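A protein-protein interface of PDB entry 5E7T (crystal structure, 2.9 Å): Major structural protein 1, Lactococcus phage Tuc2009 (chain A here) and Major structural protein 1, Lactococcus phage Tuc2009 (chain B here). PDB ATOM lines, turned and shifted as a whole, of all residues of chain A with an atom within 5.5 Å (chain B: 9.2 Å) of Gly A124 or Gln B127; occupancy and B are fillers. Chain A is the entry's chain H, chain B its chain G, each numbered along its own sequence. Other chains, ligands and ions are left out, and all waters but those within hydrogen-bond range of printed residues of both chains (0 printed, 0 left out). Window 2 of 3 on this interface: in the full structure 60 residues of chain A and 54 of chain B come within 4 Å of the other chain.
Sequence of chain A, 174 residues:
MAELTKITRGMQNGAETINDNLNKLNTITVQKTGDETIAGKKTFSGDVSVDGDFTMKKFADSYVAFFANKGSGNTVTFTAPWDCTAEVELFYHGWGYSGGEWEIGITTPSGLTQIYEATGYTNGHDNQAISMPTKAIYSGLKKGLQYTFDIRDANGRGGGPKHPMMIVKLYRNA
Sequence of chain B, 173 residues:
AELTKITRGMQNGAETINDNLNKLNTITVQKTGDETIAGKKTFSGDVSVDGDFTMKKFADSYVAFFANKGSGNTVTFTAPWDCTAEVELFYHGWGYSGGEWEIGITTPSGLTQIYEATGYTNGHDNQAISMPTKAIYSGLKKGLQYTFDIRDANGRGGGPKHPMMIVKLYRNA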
ATOM      1  N   TRP A  95      -5.704  25.393 -15.290  1.00  0.00           N
ATOM      2  CA  TRP A  95      -4.928  24.171 -15.054  1.00  0.00           C
ATOM      3  C   TRP A  95      -3.458  24.505 -14.748  1.00  0.00           C
ATOM      4  O   TRP A  95      -2.926  25.480 -15.286  1.00  0.00           O
ATOM      5  CB  TRP A  95      -5.035  23.196 -16.261  1.00  0.00           C
ATOM      6  CG  TRP A  95      -4.273  23.602 -17.501  1.00  0.00           C
ATOM      7  CD1 TRP A  95      -2.995  23.250 -17.826  1.00  0.00           C
ATOM      8  CD2 TRP A  95      -4.755  24.405 -18.591  1.00  0.00           C
ATOM      9  NE1 TRP A  95      -2.639  23.810 -19.032  1.00  0.00           N
ATOM     10  CE2 TRP A  95      -3.696  24.536 -19.517  1.00  0.00           C
ATOM     11  CE3 TRP A  95      -5.976  25.049 -18.865  1.00  0.00           C
ATOM     12  CZ2 TRP A  95      -3.826  25.261 -20.709  1.00  0.00           C
ATOM     13  CZ3 TRP A  95      -6.100  25.773 -20.043  1.00  0.00           C
ATOM     14  CH2 TRP A  95      -5.034  25.878 -20.946  1.00  0.00           C
ATOM     15  N   GLY A  96      -2.821  23.690 -13.911  1.00  0.00           N
ATOM     16  CA  GLY A  96      -1.412  23.856 -13.569  1.00  0.00           C
ATOM     17  C   GLY A  96      -0.512  23.439 -14.717  1.00  0.00           C
ATOM     18  O   GLY A  96      -0.923  22.611 -15.539  1.00  0.00           O
ATOM     19  N   GLY A  99      -0.170  19.769 -16.040  1.00  0.00           N
ATOM     20  CA  GLY A  99      -0.982  19.135 -15.009  1.00  0.00           C
ATOM     21  C   GLY A  99      -0.485  19.498 -13.622  1.00  0.00           C
ATOM     22  O   GLY A  99       0.520  20.204 -13.478  1.00  0.00           O
ATOM     23  N   GLY A 100      -1.190  19.032 -12.601  1.00  0.00           N
ATOM     24  CA  GLY A 100      -0.807  19.277 -11.215  1.00  0.00           C
ATOM     25  C   GLY A 100      -1.176  20.621 -10.616  1.00  0.00           C
ATOM     26  O   GLY A 100      -1.981  21.380 -11.168  1.00  0.00           O
ATOM     27  N   GLU A 101      -0.552  20.896  -9.459  1.00  0.00           N
ATOM     28  CA  GLU A 101      -0.731  22.045  -8.576  1.00  0.00           C
ATOM     29  C   GLU A 101      -0.615  23.423  -9.225  1.00  0.00           C
ATOM     30  O   GLU A 101       0.182  23.624 -10.145  1.00  0.00           O
ATOM     31  CB  GLU A 101       0.238  21.965  -7.384  1.00  0.00           C
ATOM     32  CG  GLU A 101       0.095  20.713  -6.534  1.00  0.00           C
ATOM     33  CD  GLU A 101       0.826  20.749  -5.204  1.00  0.00           C
ATOM     34  OE1 GLU A 101       2.065  20.931  -5.205  1.00  0.00           O
ATOM     35  OE2 GLU A 101       0.160  20.567  -4.160  1.00  0.00           O
ATOM     36  N   TYR A 121      -7.221  26.629  -5.464  1.00  0.00           N
ATOM     37  CA  TYR A 121      -6.372  25.493  -5.827  1.00  0.00           C
ATOM     38  C   TYR A 121      -6.959  24.606  -6.947  1.00  0.00           C
ATOM     39  O   TYR A 121      -8.178  24.428  -7.036  1.00  0.00           O
ATOM     40  CB  TYR A 121      -6.051  24.675  -4.553  1.00  0.00           C
ATOM     41  CG  TYR A 121      -5.178  23.454  -4.745  1.00  0.00           C
ATOM     42  CD1 TYR A 121      -3.795  23.564  -4.833  1.00  0.00           C
ATOM     43  CD2 TYR A 121      -5.730  22.175  -4.750  1.00  0.00           C
ATOM     44  CE1 TYR A 121      -2.984  22.438  -4.971  1.00  0.00           C
ATOM     45  CE2 TYR A 121      -4.931  21.043  -4.903  1.00  0.00           C
ATOM     46  CZ  TYR A 121      -3.558  21.177  -5.007  1.00  0.00           C
ATOM     47  OH  TYR A 121      -2.781  20.051  -5.146  1.00  0.00           O
ATOM     48  N   THR A 122      -6.063  24.062  -7.800  1.00  0.00           N
ATOM     49  CA  THR A 122      -6.376  23.166  -8.920  1.00  0.00           C
ATOM     50  C   THR A 122      -5.270  22.091  -9.051  1.00  0.00           C
ATOM     51  O   THR A 122      -4.124  22.346  -8.669  1.00  0.00           O
ATOM     52  CB  THR A 122      -6.680  23.973 -10.206  1.00  0.00           C
ATOM     53  OG1 THR A 122      -7.585  23.243 -11.032  1.00  0.00           O
ATOM     54  CG2 THR A 122      -5.427  24.371 -10.991  1.00  0.00           C
ATOM     55  N   ASN A 123      -5.619  20.892  -9.571  1.00  0.00           N
ATOM     56  CA  ASN A 123      -4.710  19.745  -9.721  1.00  0.00           C
ATOM     57  C   ASN A 123      -5.129  18.864 -10.915  1.00  0.00           C
ATOM     58  O   ASN A 123      -6.323  18.636 -11.118  1.00  0.00           O
ATOM     59  CB  ASN A 123      -4.726  18.915  -8.420  1.00  0.00           C
ATOM     60  CG  ASN A 123      -3.494  18.091  -8.111  1.00  0.00           C
ATOM     61  OD1 ASN A 123      -2.775  17.614  -8.995  1.00  0.00           O
ATOM     62  ND2 ASN A 123      -3.269  17.847  -6.829  1.00  0.00           N
ATOM     63  N   GLY A 124      -4.141  18.373 -11.670  1.00  0.00           N
ATOM     64  CA  GLY A 124      -4.328  17.506 -12.835  1.00  0.00           C
ATOM     65  C   GLY A 124      -5.004  18.167 -14.023  1.00  0.00           C
ATOM     66  O   GLY A 124      -4.812  19.365 -14.256  1.00  0.00           O
ATOM     67  N   HIS A 125      -5.812  17.373 -14.778  1.00  0.00           N
ATOM     68  CA  HIS A 125      -6.599  17.755 -15.966  1.00  0.00           C
ATOM     69  C   HIS A 125      -5.866  18.759 -16.914  1.00  0.00           C
ATOM     70  O   HIS A 125      -6.364  19.859 -17.173  1.00  0.00           O
ATOM     71  CB  HIS A 125      -8.004  18.259 -15.554  1.00  0.00           C
ATOM     72  CG  HIS A 125      -7.992  19.474 -14.671  1.00  0.00           C
ATOM     73  ND1 HIS A 125      -8.035  19.368 -13.295  1.00  0.00           N
ATOM     74  CD2 HIS A 125      -7.913  20.783 -15.002  1.00  0.00           C
ATOM     75  CE1 HIS A 125      -7.984  20.610 -12.840  1.00  0.00           C
ATOM     76  NE2 HIS A 125      -7.908  21.493 -13.830  1.00  0.00           N
ATOM     77  N   ASP A 126      -4.682  18.364 -17.432  1.00  0.00           N
ATOM     78  CA  ASP A 126      -3.855  19.202 -18.319  1.00  0.00           C
ATOM     79  C   ASP A 126      -4.586  19.658 -19.599  1.00  0.00           C
ATOM     80  O   ASP A 126      -5.266  18.856 -20.246  1.00  0.00           O
ATOM     81  CB  ASP A 126      -2.513  18.517 -18.655  1.00  0.00           C
ATOM     82  CG  ASP A 126      -1.544  19.374 -19.458  1.00  0.00           C
ATOM     83  OD1 ASP A 126      -1.291  20.533 -19.048  1.00  0.00           O
ATOM     84  OD2 ASP A 126      -1.030  18.881 -20.488  1.00  0.00           O
ATOM     85  N   HIS B  92     -11.577  22.721  -1.260  1.00  0.00           N
ATOM     86  CA  HIS B  92     -10.978  22.052  -2.424  1.00  0.00           C
ATOM     87  C   HIS B  92     -10.688  20.615  -1.971  1.00  0.00           C
ATOM     88  O   HIS B  92     -10.071  20.436  -0.917  1.00  0.00           O
ATOM     89  CB  HIS B  92      -9.667  22.744  -2.896  1.00  0.00           C
ATOM     90  CG  HIS B  92      -9.724  24.244  -2.983  1.00  0.00           C
ATOM     91  ND1 HIS B  92     -10.035  24.893  -4.169  1.00  0.00           N
ATOM     92  CD2 HIS B  92      -9.489  25.171  -2.029  1.00  0.00           C
ATOM     93  CE1 HIS B  92     -10.013  26.184  -3.888  1.00  0.00           C
ATOM     94  NE2 HIS B  92      -9.681  26.401  -2.617  1.00  0.00           N
ATOM     95  N   GLY B  93     -11.157  19.615  -2.722  1.00  0.00           N
ATOM     96  CA  GLY B  93     -10.950  18.216  -2.353  1.00  0.00           C
ATOM     97  C   GLY B  93     -11.342  17.173  -3.376  1.00  0.00           C
ATOM     98  O   GLY B  93     -11.486  17.478  -4.564  1.00  0.00           O
ATOM     99  N   TRP B  94     -11.492  15.914  -2.901  1.00  0.00           N
ATOM    100  CA  TRP B  94     -11.884  14.727  -3.677  1.00  0.00           C
ATOM    101  C   TRP B  94     -12.622  13.712  -2.788  1.00  0.00           C
ATOM    102  O   TRP B  94     -12.314  13.608  -1.598  1.00  0.00           O
ATOM    103  CB  TRP B  94     -10.657  14.073  -4.364  1.00  0.00           C
ATOM    104  CG  TRP B  94      -9.714  13.329  -3.446  1.00  0.00           C
ATOM    105  CD1 TRP B  94      -9.755  12.001  -3.131  1.00  0.00           C
ATOM    106  CD2 TRP B  94      -8.573  13.869  -2.757  1.00  0.00           C
ATOM    107  NE1 TRP B  94      -8.736  11.686  -2.261  1.00  0.00           N
ATOM    108  CE2 TRP B  94      -8.000  12.816  -2.006  1.00  0.00           C
ATOM    109  CE3 TRP B  94      -7.990  15.148  -2.681  1.00  0.00           C
ATOM    110  CZ2 TRP B  94      -6.860  12.996  -1.214  1.00  0.00           C
ATOM    111  CZ3 TRP B  94      -6.866  15.326  -1.888  1.00  0.00           C
ATOM    112  CH2 TRP B  94      -6.316  14.260  -1.164  1.00  0.00           C
ATOM    113  N   GLY B  95     -13.567  12.973  -3.371  1.00  0.00           N
ATOM    114  CA  GLY B  95     -14.307  11.933  -2.660  1.00  0.00           C
ATOM    115  C   GLY B  95     -13.438  10.709  -2.422  1.00  0.00           C
ATOM    116  O   GLY B  95     -12.504  10.468  -3.193  1.00  0.00           O
ATOM    117  N   GLY B  98     -12.124   8.350  -5.265  1.00  0.00           N
ATOM    118  CA  GLY B  98     -12.838   8.977  -6.367  1.00  0.00           C
ATOM    119  C   GLY B  98     -14.324   9.056  -6.076  1.00  0.00           C
ATOM    120  O   GLY B  98     -14.792   8.574  -5.039  1.00  0.00           O
ATOM    121  N   GLY B  99     -15.063   9.677  -6.980  1.00  0.00           N
ATOM    122  CA  GLY B  99     -16.506   9.799  -6.843  1.00  0.00           C
ATOM    123  C   GLY B  99     -17.035  10.892  -5.931  1.00  0.00           C
ATOM    124  O   GLY B  99     -16.309  11.804  -5.518  1.00  0.00           O
ATOM    125  N   TRP B 101     -18.971  13.340  -3.111  1.00  0.00           N
ATOM    126  CA  TRP B 101     -18.725  14.047  -1.847  1.00  0.00           C
ATOM    127  C   TRP B 101     -19.451  15.399  -1.907  1.00  0.00           C
ATOM    128  O   TRP B 101     -19.197  16.198  -2.815  1.00  0.00           O
ATOM    129  CB  TRP B 101     -17.222  14.229  -1.534  1.00  0.00           C
ATOM    130  CG  TRP B 101     -16.931  14.760  -0.151  1.00  0.00           C
ATOM    131  CD1 TRP B 101     -17.771  14.761   0.928  1.00  0.00           C
ATOM    132  CD2 TRP B 101     -15.701  15.340   0.300  1.00  0.00           C
ATOM    133  NE1 TRP B 101     -17.149  15.334   2.014  1.00  0.00           N
ATOM    134  CE2 TRP B 101     -15.875  15.694   1.658  1.00  0.00           C
ATOM    135  CE3 TRP B 101     -14.466  15.611  -0.316  1.00  0.00           C
ATOM    136  CZ2 TRP B 101     -14.852  16.272   2.419  1.00  0.00           C
ATOM    137  CZ3 TRP B 101     -13.456  16.188   0.436  1.00  0.00           C
ATOM    138  CH2 TRP B 101     -13.646  16.495   1.789  1.00  0.00           C
ATOM    139  N   THR B 121     -18.460  17.314  -5.595  1.00  0.00           N
ATOM    140  CA  THR B 121     -17.253  16.901  -6.313  1.00  0.00           C
ATOM    141  C   THR B 121     -17.388  15.418  -6.745  1.00  0.00           C
ATOM    142  O   THR B 121     -18.098  14.658  -6.085  1.00  0.00           O
ATOM    143  CB  THR B 121     -15.989  17.250  -5.508  1.00  0.00           C
ATOM    144  OG1 THR B 121     -14.902  17.481  -6.404  1.00  0.00           O
ATOM    145  CG2 THR B 121     -15.625  16.199  -4.455  1.00  0.00           C
ATOM    146  N   ASN B 122     -16.725  15.025  -7.859  1.00  0.00           N
ATOM    147  CA  ASN B 122     -16.793  13.674  -8.440  1.00  0.00           C
ATOM    148  C   ASN B 122     -15.493  13.326  -9.178  1.00  0.00           C
ATOM    149  O   ASN B 122     -14.937  14.185  -9.866  1.00  0.00           O
ATOM    150  CB  ASN B 122     -17.984  13.598  -9.424  1.00  0.00           C
ATOM    151  CG  ASN B 122     -18.601  12.231  -9.662  1.00  0.00           C
ATOM    152  OD1 ASN B 122     -17.944  11.186  -9.594  1.00  0.00           O
ATOM    153  ND2 ASN B 122     -19.878  12.223 -10.021  1.00  0.00           N
ATOM    154  N   GLY B 123     -15.048  12.069  -9.046  1.00  0.00           N
ATOM    155  CA  GLY B 123     -13.837  11.539  -9.672  1.00  0.00           C
ATOM    156  C   GLY B 123     -12.544  12.156  -9.167  1.00  0.00           C
ATOM    157  O   GLY B 123     -12.443  12.517  -7.989  1.00  0.00           O
ATOM    158  N   HIS B 124     -11.545  12.287 -10.081  1.00  0.00           N
ATOM    159  CA  HIS B 124     -10.201  12.865  -9.881  1.00  0.00           C
ATOM    160  C   HIS B 124      -9.564  12.502  -8.508  1.00  0.00           C
ATOM    161  O   HIS B 124      -9.232  13.389  -7.717  1.00  0.00           O
ATOM    162  CB  HIS B 124     -10.210  14.392 -10.135  1.00  0.00           C
ATOM    163  CG  HIS B 124     -11.117  15.162  -9.223  1.00  0.00           C
ATOM    164  ND1 HIS B 124     -12.414  15.464  -9.583  1.00  0.00           N
ATOM    165  CD2 HIS B 124     -10.887  15.645  -7.981  1.00  0.00           C
ATOM    166  CE1 HIS B 124     -12.923  16.123  -8.554  1.00  0.00           C
ATOM    167  NE2 HIS B 124     -12.042  16.251  -7.568  1.00  0.00           N
ATOM    168  N   ASP B 125      -9.390  11.183  -8.241  1.00  0.00           N
ATOM    169  CA  ASP B 125      -8.831  10.672  -6.979  1.00  0.00           C
ATOM    170  C   ASP B 125      -7.426  11.218  -6.672  1.00  0.00           C
ATOM    171  O   ASP B 125      -6.578  11.268  -7.563  1.00  0.00           O
ATOM    172  CB  ASP B 125      -8.864   9.129  -6.932  1.00  0.00           C
ATOM    173  CG  ASP B 125      -8.429   8.529  -5.602  1.00  0.00           C
ATOM    174  OD1 ASP B 125      -8.953   8.963  -4.549  1.00  0.00           O
ATOM    175  OD2 ASP B 125      -7.570   7.626  -5.613  1.00  0.00           O
ATOM    176  N   ASN B 126      -7.214  11.638  -5.398  1.00  0.00           N
ATOM    177  CA  ASN B 126      -5.989  12.223  -4.820  1.00  0.00           C
ATOM    178  C   ASN B 126      -5.477  13.452  -5.624  1.00  0.00           C
ATOM    179  O   ASN B 126      -4.282  13.598  -5.906  1.00  0.00           O
ATOM    180  CB  ASN B 126      -4.904  11.167  -4.568  1.00  0.00           C
ATOM    181  CG  ASN B 126      -5.069  10.467  -3.238  1.00  0.00           C
ATOM    182  OD1 ASN B 126      -5.849   9.520  -3.098  1.00  0.00           O
ATOM    183  ND2 ASN B 126      -4.347  10.926  -2.225  1.00  0.00           N
ATOM    184  N   GLN B 127      -6.433  14.342  -5.953  1.00  0.00           N
ATOM    185  CA  GLN B 127      -6.312  15.621  -6.662  1.00  0.00           C
ATOM    186  C   GLN B 127      -7.460  16.477  -6.092  1.00  0.00           C
ATOM    187  O   GLN B 127      -8.602  16.011  -6.095  1.00  0.00           O
ATOM    188  CB  GLN B 127      -6.518  15.436  -8.188  1.00  0.00           C
ATOM    189  CG  GLN B 127      -5.427  14.653  -8.928  1.00  0.00           C
ATOM    190  CD  GLN B 127      -5.747  14.430 -10.395  1.00  0.00           C
ATOM    191  OE1 GLN B 127      -6.866  14.073 -10.786  1.00  0.00           O
ATOM    192  NE2 GLN B 127      -4.747  14.580 -11.240  1.00  0.00           N
ATOM    193  N   ALA B 128      -7.172  17.690  -5.571  1.00  0.00           N
ATOM    194  CA  ALA B 128      -8.210  18.549  -4.978  1.00  0.00           C
ATOM    195  C   ALA B 128      -8.762  19.625  -5.932  1.00  0.00           C
ATOM    196  O   ALA B 128      -8.018  20.500  -6.384  1.00  0.00           O
ATOM    197  CB  ALA B 128      -7.708  19.172  -3.684  1.00  0.00           C
ATOM    198  N   ILE B 129     -10.072  19.544  -6.236  1.00  0.00           N
ATOM    199  CA  ILE B 129     -10.799  20.458  -7.136  1.00  0.00           C
ATOM    200  C   ILE B 129     -11.732  21.369  -6.318  1.00  0.00           C
ATOM    201  O   ILE B 129     -12.204  20.941  -5.264  1.00  0.00           O
ATOM    202  CB  ILE B 129     -11.556  19.626  -8.240  1.00  0.00           C
ATOM    203  CG1 ILE B 129     -10.580  18.966  -9.253  1.00  0.00           C
ATOM    204  CG2 ILE B 129     -12.670  20.393  -8.968  1.00  0.00           C
ATOM    205  CD1 ILE B 129      -9.668  19.890 -10.058  1.00  0.00           C
ATOM    206  N   SER B 130     -11.997  22.617  -6.801  1.00  0.00           N
ATOM    207  CA  SER B 130     -12.901  23.578  -6.144  1.00  0.00           C
ATOM    208  C   SER B 130     -14.294  22.983  -5.912  1.00  0.00           C
ATOM    209  O   SER B 130     -14.826  22.288  -6.779  1.00  0.00           O
ATOM    210  CB  SER B 130     -13.009  24.872  -6.948  1.00  0.00           C
ATOM    211  OG  SER B 130     -13.924  25.797  -6.384  1.00  0.00           O
ATOM    212  N   MET B 131     -14.832  23.202  -4.709  1.00  0.00           N
ATOM    213  CA  MET B 131     -16.147  22.740  -4.270  1.00  0.00           C
ATOM    214  C   MET B 131     -16.696  23.703  -3.182  1.00  0.00           C
ATOM    215  O   MET B 131     -16.933  23.268  -2.047  1.00  0.00           O
ATOM    216  CB  MET B 131     -16.112  21.253  -3.822  1.00  0.00           C
ATOM    217  CG  MET B 131     -15.058  20.929  -2.763  1.00  0.00           C
ATOM    218  SD  MET B 131     -14.824  19.169  -2.424  1.00  0.00           S
ATOM    219  CE  MET B 131     -16.375  18.754  -1.663  1.00  0.00           C
ATOM    220  N   GLY B 158     -12.654  12.194   1.173  1.00  0.00           N
ATOM    221  CA  GLY B 158     -11.348  11.650   0.819  1.00  0.00           C
ATOM    222  C   GLY B 158     -10.214  12.396   1.493  1.00  0.00           C
ATOM    223  O   GLY B 158      -9.354  11.782   2.133  1.00  0.00           O
ATOM    224  N   GLY B 159     -10.227  13.720   1.351  1.00  0.00           N
ATOM    225  CA  GLY B 159      -9.218  14.585   1.945  1.00  0.00           C
ATOM    226  C   GLY B 159      -9.293  16.032   1.502  1.00  0.00           C
ATOM    227  O   GLY B 159      -9.359  16.304   0.298  1.00  0.00           O
ATOM    228  N   PRO B 160      -9.251  16.994   2.459  1.00  0.00           N
ATOM    229  CA  PRO B 160      -9.294  18.417   2.076  1.00  0.00           C
ATOM    230  C   PRO B 160      -7.913  19.013   1.777  1.00  0.00           C
ATOM    231  O   PRO B 160      -6.895  18.424   2.143  1.00  0.00           O
ATOM    232  CB  PRO B 160      -9.942  19.095   3.294  1.00  0.00           C
ATOM    233  CG  PRO B 160      -9.904  18.062   4.415  1.00  0.00           C
ATOM    234  CD  PRO B 160      -9.180  16.845   3.925  1.00  0.00           C
ATOM    235  N   LYS B 161      -7.891  20.190   1.109  1.00  0.00           N
ATOM    236  CA  LYS B 161      -6.685  20.955   0.756  1.00  0.00           C
ATOM    237  C   LYS B 161      -7.041  22.439   0.549  1.00  0.00           C
ATOM    238  O   LYS B 161      -7.985  22.750  -0.180  1.00  0.00           O
ATOM    239  CB  LYS B 161      -5.977  20.363  -0.483  1.00  0.00           C
ATOM    240  CG  LYS B 161      -4.464  20.208  -0.298  1.00  0.00           C
ATOM    241  CD  LYS B 161      -3.668  21.049  -1.287  1.00  0.00           C
ATOM    242  CE  LYS B 161      -2.171  20.947  -1.088  1.00  0.00           C
ATOM    243  NZ  LYS B 161      -1.683  21.775   0.051  1.00  0.00           N
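Of the 22 printed residues of chain B, 5 touch a printed residue of chain A.
A ring nitrogen (ND1) of His B92 sits at hydrogen-bond distance from the backbone carbonyl oxygen (O) of Tyr A121, at 3.4 Å.
The side-chain hydroxyl (OG1) of Thr A122 sits close to a ring nitrogen (NE2) of His A125 (3.3 Å).
O of His B92 sits at hydrogen-bond distance from N of Lys B161.
OH of Tyr A121 sits at hydrogen-bond distance from ND2 of Asn A123.
The backbone carbonyl oxygen (O) of Asn A123 lies within hydrogen-bond range of a ring nitrogen (ND1) of His A125 (2.9 Å).
The side-chain hydroxyl of Tyr A121 sits at hydrogen-bond distance from the side-chain carboxylate of Glu A101 (3.1 Å).
The backbone carbonyl oxygen (O) of Gly B93 lies within hydrogen-bond range of the backbone NH (N) of Ile B129.
No residue of chain B comes within 4 Å of Gly A100.
Of the printed residues of chain B, Glu A101 touches Lys B161.
Of the printed residues of chain B, Tyr A121 touches His B92 (3.2 Å), Ala B128 (3.3 Å) and Lys B161 (3.7 Å).
Asn A123 touches just these residues of chain B: Gln B127 (3.8 Å), Ala B128 (3.9 Å) and Ile B129 (3.7 Å).
Printed residues of chain B within 4 Å of Gly A124: Gln B127.
Of the printed residues of chain A, His B92 touches Tyr A121 (3.2 Å).
Gln B127 touches two residues of chain A.
Of the printed residues of chain A, Ala B128 touches Tyr A121 (3.3 Å) and Asn A123 (3.9 Å).
Printed residues of chain A within 4 Å of Ile B129: Asn A123 and His A125.
Glu A101 touches Lys B161 (OE2 to CE, 3.9 Å).
Ala B128 touches Tyr A121 (O to CD2, 3.3 Å).
Lys B161 touches Tyr A121 (CD to CZ, 3.7 Å).
CA of Gln B127 touches ND2 of Asn A123, at 3.8 Å.
Asn A123 touches Ala B128.
CD1 of Ile B129 touches O of Asn A123, at 3.7 Å.
Gly A124 touches Gln B127.
Ile B129 touches His A125 (CD1 to CE1, 3.3 Å).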
